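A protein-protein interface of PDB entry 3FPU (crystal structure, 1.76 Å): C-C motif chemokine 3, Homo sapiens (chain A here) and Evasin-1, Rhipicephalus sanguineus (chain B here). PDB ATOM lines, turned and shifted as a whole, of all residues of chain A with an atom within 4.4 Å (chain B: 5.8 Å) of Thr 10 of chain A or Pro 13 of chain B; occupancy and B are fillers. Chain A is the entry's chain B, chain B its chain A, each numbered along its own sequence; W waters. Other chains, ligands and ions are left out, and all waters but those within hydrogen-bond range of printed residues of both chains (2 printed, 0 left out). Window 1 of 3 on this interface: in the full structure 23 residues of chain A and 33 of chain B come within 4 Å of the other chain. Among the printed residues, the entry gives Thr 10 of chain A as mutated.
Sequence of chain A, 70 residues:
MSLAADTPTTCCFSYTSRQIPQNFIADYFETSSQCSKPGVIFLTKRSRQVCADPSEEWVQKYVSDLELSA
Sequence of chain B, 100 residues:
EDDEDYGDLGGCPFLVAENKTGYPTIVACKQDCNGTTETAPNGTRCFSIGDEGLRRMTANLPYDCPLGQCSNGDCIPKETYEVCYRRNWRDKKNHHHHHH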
ATOM      1  N   PRO A   8      -2.224 -13.758  -2.269  1.00  0.00           N
ATOM      2  CA  PRO A   8      -1.815 -12.402  -1.889  1.00  0.00           C
ATOM      3  C   PRO A   8      -2.514 -11.301  -2.656  1.00  0.00           C
ATOM      4  O   PRO A   8      -2.885 -11.469  -3.829  1.00  0.00           O
ATOM      5  CB  PRO A   8      -0.310 -12.379  -2.216  1.00  0.00           C
ATOM      6  CG  PRO A   8       0.108 -13.808  -2.164  1.00  0.00           C
ATOM      7  CD  PRO A   8      -1.079 -14.510  -2.807  1.00  0.00           C
ATOM      8  N   THR A   9      -2.662 -10.155  -1.994  1.00  0.00           N
ATOM      9  CA  THR A   9      -3.180  -8.959  -2.644  1.00  0.00           C
ATOM     10  C   THR A   9      -2.220  -8.529  -3.765  1.00  0.00           C
ATOM     11  O   THR A   9      -1.035  -8.827  -3.718  1.00  0.00           O
ATOM     12  CB  THR A   9      -3.347  -7.768  -1.647  1.00  0.00           C
ATOM     13  OG1 THR A   9      -2.083  -7.537  -1.012  1.00  0.00           O
ATOM     14  CG2 THR A   9      -4.366  -8.151  -0.551  1.00  0.00           C
ATOM     15  N   THR A  10      -2.782  -7.818  -4.732  1.00  0.00           N
ATOM     16  CA  THR A  10      -2.078  -7.355  -5.937  1.00  0.00           C
ATOM     17  C   THR A  10      -2.447  -5.936  -6.295  1.00  0.00           C
ATOM     18  O   THR A  10      -3.452  -5.396  -5.773  1.00  0.00           O
ATOM     19  CB  THR A  10      -2.378  -8.265  -7.161  1.00  0.00           C
ATOM     20  OG1 THR A  10      -3.779  -8.205  -7.457  1.00  0.00           O
ATOM     21  CG2 THR A  10      -1.954  -9.671  -6.869  1.00  0.00           C
ATOM     22  N   CYS A  11      -1.620  -5.339  -7.170  1.00  0.00           N
ATOM     23  CA  CYS A  11      -1.974  -4.073  -7.809  1.00  0.00           C
ATOM     24  C   CYS A  11      -1.833  -4.282  -9.300  1.00  0.00           C
ATOM     25  O   CYS A  11      -1.088  -5.180  -9.743  1.00  0.00           O
ATOM     26  CB  CYS A  11      -0.989  -2.952  -7.417  1.00  0.00           C
ATOM     27  SG  CYS A  11      -1.141  -2.412  -5.605  1.00  0.00           S
ATOM     28  N   THR A  31      -8.486  -4.062  -5.813  1.00  0.00           N
ATOM     29  CA  THR A  31      -7.136  -3.826  -5.391  1.00  0.00           C
ATOM     30  C   THR A  31      -7.184  -2.637  -4.430  1.00  0.00           C
ATOM     31  O   THR A  31      -8.163  -1.896  -4.418  1.00  0.00           O
ATOM     32  CB  THR A  31      -6.180  -3.532  -6.566  1.00  0.00           C
ATOM     33  OG1 THR A  31      -6.615  -2.369  -7.279  1.00  0.00           O
ATOM     34  CG2 THR A  31      -6.148  -4.758  -7.558  1.00  0.00           C
ATOM     35  N   CYS A  35      -2.868   1.429  -4.132  1.00  0.00           N
ATOM     36  CA  CYS A  35      -2.117   1.082  -5.338  1.00  0.00           C
ATOM     37  C   CYS A  35      -1.959   2.350  -6.210  1.00  0.00           C
ATOM     38  O   CYS A  35      -2.781   3.244  -6.117  1.00  0.00           O
ATOM     39  CB  CYS A  35      -2.887   0.040  -6.172  1.00  0.00           C
ATOM     40  SG  CYS A  35      -2.974  -1.627  -5.420  1.00  0.00           S
ATOM     41  N   ILE A  41      -9.758  -7.042  -9.925  1.00  0.00           N
ATOM     42  CA  ILE A  41      -9.183  -8.346 -10.305  1.00  0.00           C
ATOM     43  C   ILE A  41     -10.357  -9.297 -10.506  1.00  0.00           C
ATOM     44  O   ILE A  41     -11.160  -9.497  -9.594  1.00  0.00           O
ATOM     45  CB  ILE A  41      -8.361  -8.976  -9.149  1.00  0.00           C
ATOM     46  CG1 ILE A  41      -7.169  -8.098  -8.736  1.00  0.00           C
ATOM     47  CG2 ILE A  41      -7.952 -10.386  -9.525  1.00  0.00           C
ATOM     48  CD1 ILE A  41      -6.163  -7.751  -9.813  1.00  0.00           C
ATOM     49  N   GLN A  49      -6.158 -14.877 -12.195  1.00  0.00           N
ATOM     50  CA  GLN A  49      -6.517 -13.530 -11.735  1.00  0.00           C
ATOM     51  C   GLN A  49      -6.067 -12.530 -12.801  1.00  0.00           C
ATOM     52  O   GLN A  49      -4.891 -12.552 -13.245  1.00  0.00           O
ATOM     53  CB  GLN A  49      -5.895 -13.259 -10.337  1.00  0.00           C
ATOM     54  CG  GLN A  49      -6.550 -14.133  -9.312  1.00  0.00           C
ATOM     55  CD  GLN A  49      -6.066 -13.938  -7.884  1.00  0.00           C
ATOM     56  OE1 GLN A  49      -5.693 -12.835  -7.491  1.00  0.00           O
ATOM     57  NE2 GLN A  49      -6.109 -15.017  -7.092  1.00  0.00           N
ATOM     58  N   VAL A  50      -7.011 -11.681 -13.237  1.00  0.00           N
ATOM     59  CA  VAL A  50      -6.811 -10.751 -14.360  1.00  0.00           C
ATOM     60  C   VAL A  50      -7.168  -9.299 -13.972  1.00  0.00           C
ATOM     61  O   VAL A  50      -8.236  -9.064 -13.447  1.00  0.00           O
ATOM     62  CB  VAL A  50      -7.651 -11.147 -15.594  1.00  0.00           C
ATOM     63  CG1 VAL A  50      -9.072 -11.315 -15.260  1.00  0.00           C
ATOM     64  CG2 VAL A  50      -7.479 -10.115 -16.694  1.00  0.00           C
ATOM     65  N   CYS A  51      -6.277  -8.358 -14.232  1.00  0.00           N
ATOM     66  CA  CYS A  51      -6.602  -6.925 -13.995  1.00  0.00           C
ATOM     67  C   CYS A  51      -7.627  -6.348 -14.963  1.00  0.00           C
ATOM     68  O   CYS A  51      -7.487  -6.505 -16.165  1.00  0.00           O
ATOM     69  CB  CYS A  51      -5.351  -6.079 -14.098  1.00  0.00           C
ATOM     70  SG  CYS A  51      -4.268  -6.319 -12.718  1.00  0.00           S
ATOM     71  N   GLY B  11      -3.243  -8.289 -18.627  1.00  0.00           N
ATOM     72  CA  GLY B  11      -3.608  -7.776 -17.305  1.00  0.00           C
ATOM     73  C   GLY B  11      -2.953  -8.558 -16.188  1.00  0.00           C
ATOM     74  O   GLY B  11      -3.643  -8.961 -15.269  1.00  0.00           O
ATOM     75  N   CYS B  12      -1.645  -8.811 -16.260  1.00  0.00           N
ATOM     76  CA  CYS B  12      -0.989  -9.569 -15.193  1.00  0.00           C
ATOM     77  C   CYS B  12      -1.003  -8.741 -13.906  1.00  0.00           C
ATOM     78  O   CYS B  12      -0.441  -7.626 -13.868  1.00  0.00           O
ATOM     79  CB  CYS B  12       0.461  -9.948 -15.526  1.00  0.00           C
ATOM     80  SG  CYS B  12       0.750 -10.685 -17.203  1.00  0.00           S
ATOM     81  N   PRO B  13      -1.640  -9.270 -12.852  1.00  0.00           N
ATOM     82  CA  PRO B  13      -1.497  -8.522 -11.583  1.00  0.00           C
ATOM     83  C   PRO B  13      -0.106  -8.712 -11.004  1.00  0.00           C
ATOM     84  O   PRO B  13       0.535  -9.805 -11.140  1.00  0.00           O
ATOM     85  CB  PRO B  13      -2.544  -9.196 -10.658  1.00  0.00           C
ATOM     86  CG  PRO B  13      -3.437 -10.072 -11.598  1.00  0.00           C
ATOM     87  CD  PRO B  13      -2.472 -10.471 -12.686  1.00  0.00           C
ATOM     88  N   PHE B  14       0.352  -7.664 -10.288  1.00  0.00           N
ATOM     89  CA  PHE B  14       1.597  -7.726  -9.590  1.00  0.00           C
ATOM     90  C   PHE B  14       1.304  -7.971  -8.110  1.00  0.00           C
ATOM     91  O   PHE B  14       0.595  -7.154  -7.532  1.00  0.00           O
ATOM     92  CB  PHE B  14       2.296  -6.386  -9.724  1.00  0.00           C
ATOM     93  CG  PHE B  14       3.018  -6.219 -11.039  1.00  0.00           C
ATOM     94  CD1 PHE B  14       4.400  -6.269 -11.072  1.00  0.00           C
ATOM     95  CD2 PHE B  14       2.304  -6.089 -12.213  1.00  0.00           C
ATOM     96  CE1 PHE B  14       5.092  -6.138 -12.312  1.00  0.00           C
ATOM     97  CE2 PHE B  14       2.990  -5.936 -13.453  1.00  0.00           C
ATOM     98  CZ  PHE B  14       4.368  -5.982 -13.452  1.00  0.00           C
ATOM     99  N   LEU B  15       1.864  -9.059  -7.551  1.00  0.00           N
ATOM    100  CA  LEU B  15       1.808  -9.344  -6.087  1.00  0.00           C
ATOM    101  C   LEU B  15       2.462  -8.192  -5.357  1.00  0.00           C
ATOM    102  O   LEU B  15       3.460  -7.661  -5.849  1.00  0.00           O
ATOM    103  CB  LEU B  15       2.603 -10.611  -5.746  1.00  0.00           C
ATOM    104  CG  LEU B  15       2.004 -11.894  -6.361  1.00  0.00           C
ATOM    105  CD1 LEU B  15       2.692 -13.048  -5.705  1.00  0.00           C
ATOM    106  CD2 LEU B  15       0.532 -11.960  -6.082  1.00  0.00           C
ATOM    107  N   VAL B  16       1.876  -7.800  -4.232  1.00  0.00           N
ATOM    108  CA  VAL B  16       2.470  -6.733  -3.412  1.00  0.00           C
ATOM    109  C   VAL B  16       2.610  -7.215  -1.975  1.00  0.00           C
ATOM    110  O   VAL B  16       1.883  -8.114  -1.535  1.00  0.00           O
ATOM    111  CB  VAL B  16       1.629  -5.464  -3.467  1.00  0.00           C
ATOM    112  CG1 VAL B  16       1.656  -4.906  -4.926  1.00  0.00           C
ATOM    113  CG2 VAL B  16       0.128  -5.691  -2.940  1.00  0.00           C
ATOM    114  N   GLN B  31       6.066  -9.529 -14.370  1.00  0.00           N
ATOM    115  CA  GLN B  31       5.092 -10.599 -14.130  1.00  0.00           C
ATOM    116  C   GLN B  31       4.729 -11.302 -15.420  1.00  0.00           C
ATOM    117  O   GLN B  31       4.495 -10.633 -16.417  1.00  0.00           O
ATOM    118  CB  GLN B  31       3.792 -10.040 -13.541  1.00  0.00           C
ATOM    119  CG  GLN B  31       3.891  -9.494 -12.140  1.00  0.00           C
ATOM    120  CD  GLN B  31       3.885 -10.555 -11.022  1.00  0.00           C
ATOM    121  OE1 GLN B  31       3.974 -10.214  -9.812  1.00  0.00           O
ATOM    122  NE2 GLN B  31       3.795 -11.835 -11.405  1.00  0.00           N
ATOM    123  N   CYS B  33       1.947 -13.886 -17.301  1.00  0.00           N
ATOM    124  CA  CYS B  33       0.639 -14.525 -17.186  1.00  0.00           C
ATOM    125  C   CYS B  33       0.259 -15.032 -18.578  1.00  0.00           C
ATOM    126  O   CYS B  33       0.233 -14.251 -19.524  1.00  0.00           O
ATOM    127  CB  CYS B  33      -0.381 -13.550 -16.581  1.00  0.00           C
ATOM    128  SG  CYS B  33      -0.758 -12.035 -17.482  1.00  0.00           S
ATOM    129  N   TRP B  89      -6.330 -11.655   0.108  1.00  0.00           N
ATOM    130  CA  TRP B  89      -7.617 -11.005  -0.132  1.00  0.00           C
ATOM    131  C   TRP B  89      -8.580 -11.099   1.057  1.00  0.00           C
ATOM    132  O   TRP B  89      -9.302 -10.150   1.336  1.00  0.00           O
ATOM    133  CB  TRP B  89      -8.300 -11.610  -1.369  1.00  0.00           C
ATOM    134  CG  TRP B  89      -7.495 -11.375  -2.629  1.00  0.00           C
ATOM    135  CD1 TRP B  89      -6.962 -12.328  -3.434  1.00  0.00           C
ATOM    136  CD2 TRP B  89      -7.188 -10.109  -3.241  1.00  0.00           C
ATOM    137  NE1 TRP B  89      -6.323 -11.746  -4.513  1.00  0.00           N
ATOM    138  CE2 TRP B  89      -6.445 -10.387  -4.418  1.00  0.00           C
ATOM    139  CE3 TRP B  89      -7.470  -8.766  -2.923  1.00  0.00           C
ATOM    140  CZ2 TRP B  89      -5.958  -9.374  -5.266  1.00  0.00           C
ATOM    141  CZ3 TRP B  89      -6.968  -7.752  -3.779  1.00  0.00           C
ATOM    142  CH2 TRP B  89      -6.237  -8.072  -4.929  1.00  0.00           C
HETATM  143  O   HOH W   1      -3.948 -12.478 -15.709  1.00  0.00           O
HETATM  144  O   HOH W   2       0.194  -8.711   0.357  1.00  0.00           O
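Printed residues of chain B within 4 Å of Thr 9 of chain A: Leu 15, Val 16 and Trp 89.
Thr 10 of chain A touches four residues of chain B.
Of the printed residues of chain B, Cys 11 of chain A touches Pro 13, Phe 14 and Val 16.
Cys 35 of chain A touches none of the printed residues of chain B.
Of the printed residues of chain B, Gln 49 of chain A touches Pro 13 and Trp 89.
Printed residues of chain A within 4 Å of Gly 11 of chain B: Val 50 (3.8 Å) and Cys 51 (2.9 Å).
Of the printed residues of chain A, Pro 13 of chain B touches Thr 10, Cys 11, Ile 41, Gln 49 and Cys 51.
The nearest residue of chain B that does not touch Thr 10 of chain A is Val 16 of chain B (4.03 Å).
The nearest printed residue of chain B that does not touch Pro 8 of chain A is Val 16 of chain B (4.8 Å).
The side-chain sulfur (SG) of Cys 11 of chain A forms a disulfide with the side-chain sulfur (SG) of Cys 35 of chain A, 2.0 Å away.
The side-chain sulfur of Cys 12 of chain B forms a disulfide with the side-chain sulfur of Cys 33 of chain B (2.0 Å).
The backbone NH of Leu 15 of chain B sits at hydrogen-bond distance from the side-chain amide oxygen of Gln 31 of chain B (3.3 Å).
O of Thr 9 of chain A is in hydrogen-bond range of N of Val 16 of chain B (3.1 Å).
The indole nitrogen (NE1) of Trp 89 of chain B sits at hydrogen-bond distance from the side-chain amide oxygen (OE1) of Gln 49 of chain A (3.2 Å).
O of Phe 14 of chain B is in hydrogen-bond range of N of Cys 11 of chain A (2.9 Å).
O of Gly 11 of chain B lies within hydrogen-bond range of N of Cys 51 of chain A.
Of the 9 printed residues of chain B, 6 touch a printed residue of chain A.
Along chain A the printed residues that touch a printed residue of chain B span positions 8 to 51.
Among the printed residues, 19 pairs touch across the chains.
Among the printed residues, no Asp or Glu carboxylate lies within 4 Å of a Lys or Arg side-chain nitrogen of the other chain.
Water W2 lies within hydrogen-bond range of O of Val 16 of chain B (2.6 Å) and OG1 of Thr 9 of chain A (2.9 Å).
Water W1 bridges the backbone carbonyl oxygen of Gln 49 of chain A (2.6 Å) and the side-chain sulfur of Cys 33 of chain B (3.7 Å).
Pro 8 of chain A touches Leu 15 of chain B.
O of Pro 8 of chain A touches NE1 of Trp 89 of chain B (3.5 Å).
Leu 15 of chain B touches Thr 9 of chain A (CA to O, 3.7 Å).
CA of Thr 9 of chain A touches CZ2 of Trp 89 of chain B, at 3.8 Å.
CA of Thr 10 of chain A touches O of Phe 14 of chain B (3.1 Å).
Thr 10 of chain A touches Leu 15 of chain B.
Ile 41 of chain A touches Pro 13 of chain B (CD1 to CB, 3.99 Å).
CD of Pro 13 of chain B touches O of Gln 49 of chain A, 3.2 Å away.
Gly 11 of chain B touches Val 50 of chain A (O to CA, 3.8 Å).
SG of Cys 51 of chain A touches CA of Pro 13 of chain B, 3.7 Å away.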
